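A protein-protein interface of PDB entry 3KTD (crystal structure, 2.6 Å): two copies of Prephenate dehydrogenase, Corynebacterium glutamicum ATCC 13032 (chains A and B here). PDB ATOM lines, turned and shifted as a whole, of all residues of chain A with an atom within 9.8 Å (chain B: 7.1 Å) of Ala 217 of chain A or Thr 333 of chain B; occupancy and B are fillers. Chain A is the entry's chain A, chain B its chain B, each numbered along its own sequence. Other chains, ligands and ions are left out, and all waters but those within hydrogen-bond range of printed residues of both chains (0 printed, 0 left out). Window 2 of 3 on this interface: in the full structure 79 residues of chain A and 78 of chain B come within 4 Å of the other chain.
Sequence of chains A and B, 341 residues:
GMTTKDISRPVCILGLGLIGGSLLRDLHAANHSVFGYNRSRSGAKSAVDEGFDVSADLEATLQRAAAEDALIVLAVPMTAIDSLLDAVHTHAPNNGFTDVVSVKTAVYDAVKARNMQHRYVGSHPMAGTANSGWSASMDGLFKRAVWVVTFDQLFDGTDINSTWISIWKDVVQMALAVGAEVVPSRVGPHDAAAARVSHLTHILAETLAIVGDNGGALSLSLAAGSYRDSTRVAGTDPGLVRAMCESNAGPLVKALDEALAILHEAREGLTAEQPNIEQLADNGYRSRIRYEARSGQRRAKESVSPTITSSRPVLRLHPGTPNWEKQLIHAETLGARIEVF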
ATOM      1  N   VAL A 211      -8.316 -22.884   0.074  1.00  0.00           N
ATOM      2  CA  VAL A 211      -7.629 -23.454  -1.091  1.00  0.00           C
ATOM      3  C   VAL A 211      -8.546 -23.502  -2.321  1.00  0.00           C
ATOM      4  O   VAL A 211      -8.092 -23.306  -3.454  1.00  0.00           O
ATOM      5  CB  VAL A 211      -7.044 -24.852  -0.803  1.00  0.00           C
ATOM      6  CG1 VAL A 211      -6.380 -25.439  -2.064  1.00  0.00           C
ATOM      7  CG2 VAL A 211      -6.036 -24.779   0.347  1.00  0.00           C
ATOM      8  N   GLY A 212      -9.831 -23.746  -2.093  1.00  0.00           N
ATOM      9  CA  GLY A 212     -10.814 -23.745  -3.175  1.00  0.00           C
ATOM     10  C   GLY A 212     -11.089 -22.343  -3.683  1.00  0.00           C
ATOM     11  O   GLY A 212     -11.099 -22.100  -4.898  1.00  0.00           O
ATOM     12  N   ASP A 213     -11.304 -21.422  -2.747  1.00  0.00           N
ATOM     13  CA  ASP A 213     -11.523 -20.019  -3.079  1.00  0.00           C
ATOM     14  C   ASP A 213     -10.319 -19.441  -3.829  1.00  0.00           C
ATOM     15  O   ASP A 213     -10.490 -18.660  -4.761  1.00  0.00           O
ATOM     16  CB  ASP A 213     -11.794 -19.196  -1.820  1.00  0.00           C
ATOM     17  CG  ASP A 213     -11.960 -17.711  -2.118  1.00  0.00           C
ATOM     18  OD1 ASP A 213     -12.938 -17.327  -2.799  1.00  0.00           O
ATOM     19  OD2 ASP A 213     -11.110 -16.922  -1.656  1.00  0.00           O
ATOM     20  N   ASN A 214      -9.110 -19.835  -3.422  1.00  0.00           N
ATOM     21  CA  ASN A 214      -7.882 -19.408  -4.101  1.00  0.00           C
ATOM     22  C   ASN A 214      -7.895 -19.754  -5.579  1.00  0.00           C
ATOM     23  O   ASN A 214      -7.288 -19.049  -6.383  1.00  0.00           O
ATOM     24  CB  ASN A 214      -6.634 -20.035  -3.463  1.00  0.00           C
ATOM     25  CG  ASN A 214      -6.297 -19.448  -2.092  1.00  0.00           C
ATOM     26  OD1 ASN A 214      -6.926 -18.498  -1.607  1.00  0.00           O
ATOM     27  ND2 ASN A 214      -5.291 -20.028  -1.459  1.00  0.00           N
ATOM     28  N   GLY A 215      -8.582 -20.839  -5.934  1.00  0.00           N
ATOM     29  CA  GLY A 215      -8.670 -21.290  -7.330  1.00  0.00           C
ATOM     30  C   GLY A 215      -9.501 -20.399  -8.246  1.00  0.00           C
ATOM     31  O   GLY A 215      -9.478 -20.572  -9.471  1.00  0.00           O
ATOM     32  N   GLY A 216     -10.251 -19.463  -7.663  1.00  0.00           N
ATOM     33  CA  GLY A 216     -11.041 -18.525  -8.438  1.00  0.00           C
ATOM     34  C   GLY A 216     -12.317 -19.111  -9.003  1.00  0.00           C
ATOM     35  O   GLY A 216     -12.839 -20.106  -8.489  1.00  0.00           O
ATOM     36  N   ALA A 217     -12.797 -18.503 -10.091  1.00  0.00           N
ATOM     37  CA  ALA A 217     -14.115 -18.810 -10.674  1.00  0.00           C
ATOM     38  C   ALA A 217     -14.316 -20.274 -11.076  1.00  0.00           C
ATOM     39  O   ALA A 217     -15.297 -20.911 -10.671  1.00  0.00           O
ATOM     40  CB  ALA A 217     -14.397 -17.888 -11.861  1.00  0.00           C
ATOM     41  N   LEU A 218     -13.392 -20.810 -11.859  1.00  0.00           N
ATOM     42  CA  LEU A 218     -13.529 -22.184 -12.314  1.00  0.00           C
ATOM     43  C   LEU A 218     -13.631 -23.146 -11.116  1.00  0.00           C
ATOM     44  O   LEU A 218     -14.500 -24.016 -11.090  1.00  0.00           O
ATOM     45  CB  LEU A 218     -12.378 -22.564 -13.244  1.00  0.00           C
ATOM     46  CG  LEU A 218     -12.572 -23.827 -14.087  1.00  0.00           C
ATOM     47  CD1 LEU A 218     -13.879 -23.776 -14.871  1.00  0.00           C
ATOM     48  CD2 LEU A 218     -11.383 -24.040 -15.030  1.00  0.00           C
ATOM     49  N   SER A 219     -12.785 -22.965 -10.107  1.00  0.00           N
ATOM     50  CA  SER A 219     -12.775 -23.884  -8.972  1.00  0.00           C
ATOM     51  C   SER A 219     -14.100 -23.909  -8.215  1.00  0.00           C
ATOM     52  O   SER A 219     -14.650 -24.970  -7.939  1.00  0.00           O
ATOM     53  CB  SER A 219     -11.630 -23.552  -8.016  1.00  0.00           C
ATOM     54  OG  SER A 219     -10.397 -23.967  -8.576  1.00  0.00           O
ATOM     55  N   LEU A 220     -14.614 -22.738  -7.897  1.00  0.00           N
ATOM     56  CA  LEU A 220     -15.869 -22.653  -7.180  1.00  0.00           C
ATOM     57  C   LEU A 220     -17.032 -23.166  -8.036  1.00  0.00           C
ATOM     58  O   LEU A 220     -18.014 -23.688  -7.496  1.00  0.00           O
ATOM     59  CB  LEU A 220     -16.114 -21.218  -6.702  1.00  0.00           C
ATOM     60  CG  LEU A 220     -15.051 -20.640  -5.749  1.00  0.00           C
ATOM     61  CD1 LEU A 220     -15.396 -19.201  -5.380  1.00  0.00           C
ATOM     62  CD2 LEU A 220     -14.891 -21.493  -4.491  1.00  0.00           C
ATOM     63  N   SER A 221     -16.910 -23.037  -9.359  1.00  0.00           N
ATOM     64  CA  SER A 221     -17.932 -23.527 -10.292  1.00  0.00           C
ATOM     65  C   SER A 221     -17.920 -25.048 -10.353  1.00  0.00           C
ATOM     66  O   SER A 221     -18.970 -25.683 -10.318  1.00  0.00           O
ATOM     67  CB  SER A 221     -17.702 -22.962 -11.703  1.00  0.00           C
ATOM     68  OG  SER A 221     -18.759 -23.303 -12.593  1.00  0.00           O
ATOM     69  N   LEU A 222     -16.725 -25.629 -10.442  1.00  0.00           N
ATOM     70  CA  LEU A 222     -16.584 -27.087 -10.542  1.00  0.00           C
ATOM     71  C   LEU A 222     -16.728 -27.836  -9.215  1.00  0.00           C
ATOM     72  O   LEU A 222     -16.832 -29.060  -9.206  1.00  0.00           O
ATOM     73  CB  LEU A 222     -15.254 -27.468 -11.198  1.00  0.00           C
ATOM     74  CG  LEU A 222     -14.966 -26.943 -12.613  1.00  0.00           C
ATOM     75  CD1 LEU A 222     -13.729 -27.652 -13.165  1.00  0.00           C
ATOM     76  CD2 LEU A 222     -16.148 -27.121 -13.546  1.00  0.00           C
ATOM     77  N   ALA A 223     -16.733 -27.126  -8.096  1.00  0.00           N
ATOM     78  CA  ALA A 223     -16.870 -27.804  -6.817  1.00  0.00           C
ATOM     79  C   ALA A 223     -18.193 -28.559  -6.818  1.00  0.00           C
ATOM     80  O   ALA A 223     -19.169 -28.080  -7.390  1.00  0.00           O
ATOM     81  CB  ALA A 223     -16.811 -26.822  -5.689  1.00  0.00           C
ATOM     82  N   PRO B 184     -17.242 -25.129 -20.159  1.00  0.00           N
ATOM     83  CA  PRO B 184     -16.111 -25.521 -20.987  1.00  0.00           C
ATOM     84  C   PRO B 184     -14.807 -25.247 -20.265  1.00  0.00           C
ATOM     85  O   PRO B 184     -14.758 -24.367 -19.416  1.00  0.00           O
ATOM     86  CB  PRO B 184     -16.248 -24.619 -22.207  1.00  0.00           C
ATOM     87  CG  PRO B 184     -16.857 -23.388 -21.672  1.00  0.00           C
ATOM     88  CD  PRO B 184     -17.715 -23.776 -20.495  1.00  0.00           C
ATOM     89  N   ARG B 186     -10.146 -26.129 -20.590  1.00  0.00           N
ATOM     90  CA  ARG B 186      -8.986 -26.833 -21.128  1.00  0.00           C
ATOM     91  C   ARG B 186      -8.421 -27.746 -20.042  1.00  0.00           C
ATOM     92  O   ARG B 186      -8.818 -27.633 -18.892  1.00  0.00           O
ATOM     93  CB  ARG B 186      -7.954 -25.826 -21.630  1.00  0.00           C
ATOM     94  CG  ARG B 186      -8.480 -25.001 -22.800  1.00  0.00           C
ATOM     95  CD  ARG B 186      -7.501 -23.951 -23.233  1.00  0.00           C
ATOM     96  NE  ARG B 186      -7.360 -22.890 -22.250  1.00  0.00           N
ATOM     97  CZ  ARG B 186      -6.477 -21.902 -22.343  1.00  0.00           C
ATOM     98  NH1 ARG B 186      -5.648 -21.838 -23.383  1.00  0.00           N
ATOM     99  NH2 ARG B 186      -6.417 -20.973 -21.395  1.00  0.00           N
ATOM    100  N   LEU B 328     -15.097 -19.268 -25.474  1.00  0.00           N
ATOM    101  CA  LEU B 328     -14.884 -20.469 -24.649  1.00  0.00           C
ATOM    102  C   LEU B 328     -13.900 -20.164 -23.523  1.00  0.00           C
ATOM    103  O   LEU B 328     -14.103 -20.586 -22.394  1.00  0.00           O
ATOM    104  CB  LEU B 328     -14.393 -21.666 -25.478  1.00  0.00           C
ATOM    105  CG  LEU B 328     -15.387 -22.367 -26.416  1.00  0.00           C
ATOM    106  CD1 LEU B 328     -14.730 -23.558 -27.105  1.00  0.00           C
ATOM    107  CD2 LEU B 328     -16.626 -22.821 -25.669  1.00  0.00           C
ATOM    108  N   ILE B 329     -12.840 -19.425 -23.836  1.00  0.00           N
ATOM    109  CA  ILE B 329     -11.897 -18.946 -22.821  1.00  0.00           C
ATOM    110  C   ILE B 329     -12.604 -18.049 -21.809  1.00  0.00           C
ATOM    111  O   ILE B 329     -12.299 -18.088 -20.626  1.00  0.00           O
ATOM    112  CB  ILE B 329     -10.723 -18.156 -23.464  1.00  0.00           C
ATOM    113  CG1 ILE B 329      -9.811 -19.101 -24.254  1.00  0.00           C
ATOM    114  CG2 ILE B 329      -9.916 -17.399 -22.409  1.00  0.00           C
ATOM    115  CD1 ILE B 329      -9.169 -20.190 -23.418  1.00  0.00           C
ATOM    116  N   HIS B 330     -13.549 -17.244 -22.287  1.00  0.00           N
ATOM    117  CA  HIS B 330     -14.312 -16.346 -21.426  1.00  0.00           C
ATOM    118  C   HIS B 330     -15.111 -17.165 -20.419  1.00  0.00           C
ATOM    119  O   HIS B 330     -15.070 -16.890 -19.217  1.00  0.00           O
ATOM    120  CB  HIS B 330     -15.227 -15.446 -22.267  1.00  0.00           C
ATOM    121  CG  HIS B 330     -15.834 -14.306 -21.506  1.00  0.00           C
ATOM    122  ND1 HIS B 330     -17.029 -13.722 -21.872  1.00  0.00           N
ATOM    123  CD2 HIS B 330     -15.423 -13.652 -20.393  1.00  0.00           C
ATOM    124  CE1 HIS B 330     -17.317 -12.748 -21.027  1.00  0.00           C
ATOM    125  NE2 HIS B 330     -16.361 -12.688 -20.116  1.00  0.00           N
ATOM    126  N   ALA B 331     -15.812 -18.187 -20.910  1.00  0.00           N
ATOM    127  CA  ALA B 331     -16.578 -19.093 -20.048  1.00  0.00           C
ATOM    128  C   ALA B 331     -15.677 -19.783 -19.041  1.00  0.00           C
ATOM    129  O   ALA B 331     -16.054 -19.976 -17.885  1.00  0.00           O
ATOM    130  CB  ALA B 331     -17.297 -20.127 -20.875  1.00  0.00           C
ATOM    131  N   GLU B 332     -14.485 -20.151 -19.492  1.00  0.00           N
ATOM    132  CA  GLU B 332     -13.508 -20.829 -18.644  1.00  0.00           C
ATOM    133  C   GLU B 332     -13.056 -19.946 -17.478  1.00  0.00           C
ATOM    134  O   GLU B 332     -13.004 -20.403 -16.334  1.00  0.00           O
ATOM    135  CB  GLU B 332     -12.300 -21.240 -19.484  1.00  0.00           C
ATOM    136  CG  GLU B 332     -11.279 -22.121 -18.790  1.00  0.00           C
ATOM    137  CD  GLU B 332     -10.032 -22.271 -19.630  1.00  0.00           C
ATOM    138  OE1 GLU B 332      -9.224 -21.312 -19.663  1.00  0.00           O
ATOM    139  OE2 GLU B 332      -9.865 -23.340 -20.259  1.00  0.00           O
ATOM    140  N   THR B 333     -12.724 -18.688 -17.770  1.00  0.00           N
ATOM    141  CA  THR B 333     -12.303 -17.751 -16.728  1.00  0.00           C
ATOM    142  C   THR B 333     -13.439 -17.500 -15.739  1.00  0.00           C
ATOM    143  O   THR B 333     -13.218 -17.425 -14.524  1.00  0.00           O
ATOM    144  CB  THR B 333     -11.841 -16.415 -17.317  1.00  0.00           C
ATOM    145  OG1 THR B 333     -10.734 -16.645 -18.187  1.00  0.00           O
ATOM    146  CG2 THR B 333     -11.407 -15.461 -16.218  1.00  0.00           C
ATOM    147  N   LEU B 334     -14.649 -17.388 -16.281  1.00  0.00           N
ATOM    148  CA  LEU B 334     -15.849 -17.139 -15.496  1.00  0.00           C
ATOM    149  C   LEU B 334     -16.414 -18.385 -14.822  1.00  0.00           C
ATOM    150  O   LEU B 334     -17.167 -18.270 -13.856  1.00  0.00           O
ATOM    151  CB  LEU B 334     -16.927 -16.529 -16.396  1.00  0.00           C
ATOM    152  CG  LEU B 334     -16.716 -15.072 -16.819  1.00  0.00           C
ATOM    153  CD1 LEU B 334     -17.589 -14.732 -18.006  1.00  0.00           C
ATOM    154  CD2 LEU B 334     -16.999 -14.135 -15.667  1.00  0.00           C
ATOM    155  N   GLY B 335     -16.063 -19.566 -15.326  1.00  0.00           N
ATOM    156  CA  GLY B 335     -16.660 -20.810 -14.838  1.00  0.00           C
ATOM    157  C   GLY B 335     -18.136 -20.839 -15.209  1.00  0.00           C
ATOM    158  O   GLY B 335     -18.965 -21.437 -14.515  1.00  0.00           O
ATOM    159  N   ALA B 336     -18.453 -20.181 -16.322  1.00  0.00           N
ATOM    160  CA  ALA B 336     -19.825 -20.030 -16.773  1.00  0.00           C
ATOM    161  C   ALA B 336     -20.268 -21.256 -17.543  1.00  0.00           C
ATOM    162  O   ALA B 336     -19.445 -21.954 -18.137  1.00  0.00           O
ATOM    163  CB  ALA B 336     -19.951 -18.798 -17.650  1.00  0.00           C
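OG of Ser 221 of chain A sits at hydrogen-bond distance from O of Gly 335 of chain B, at 2.7 Å.
The backbone carbonyl oxygen of Ile 329 of chain B lies within hydrogen-bond range of the side-chain hydroxyl of Thr 333 of chain B (3.2 Å).
NE of Arg 186 of chain B lies within salt-bridge range of OE2 of Glu 332 of chain B.
CB of Ala 217 of chain A touches O of Thr 333 of chain B, 2.9 Å away.
Leu 334 of chain B touches Ala 217 of chain A (O to CB, 3.4 Å).
Leu 218 of chain A touches Glu 332 of chain B.
Of chain A, only Ala 217 (2.9 Å) comes within 4 Å of Thr 333 of chain B.
No residue of chain A comes within 4 Å of Ala 331 of chain B.
Of the printed residues of chain A, Glu 332 of chain B touches Leu 218.
Of the printed residues of chain B, Leu 218 of chain A touches Glu 332.
Of the printed residues of chain B, Ser 221 of chain A touches Gly 335.
The nearest printed residue of chain B that does not touch Ser 221 of chain A is Ala 336 of chain B (4.9 Å).
Of the 11 printed residues of chain B, 4 touch a printed residue of chain A.
Printed residues of chain B that touch a printed residue of chain A: Glu 332, Thr 333, Leu 334 and Gly 335.
Printed residues of chain A that touch a printed residue of chain B: Ala 217, Leu 218 and Ser 221.
Hydrophobic or aromatic side chains of chain A within 4 Å of the printed part of chain B: Ala 217 and Leu 218.
Among the printed residues, no Asp or Glu carboxylate lies within 4 Å of a Lys or Arg side-chain nitrogen of the other chain.
No position is printed for both chains.
Of the 4 pairs that touch across the chains among the printed residues, none has its exchanged pair printed and touching as well.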
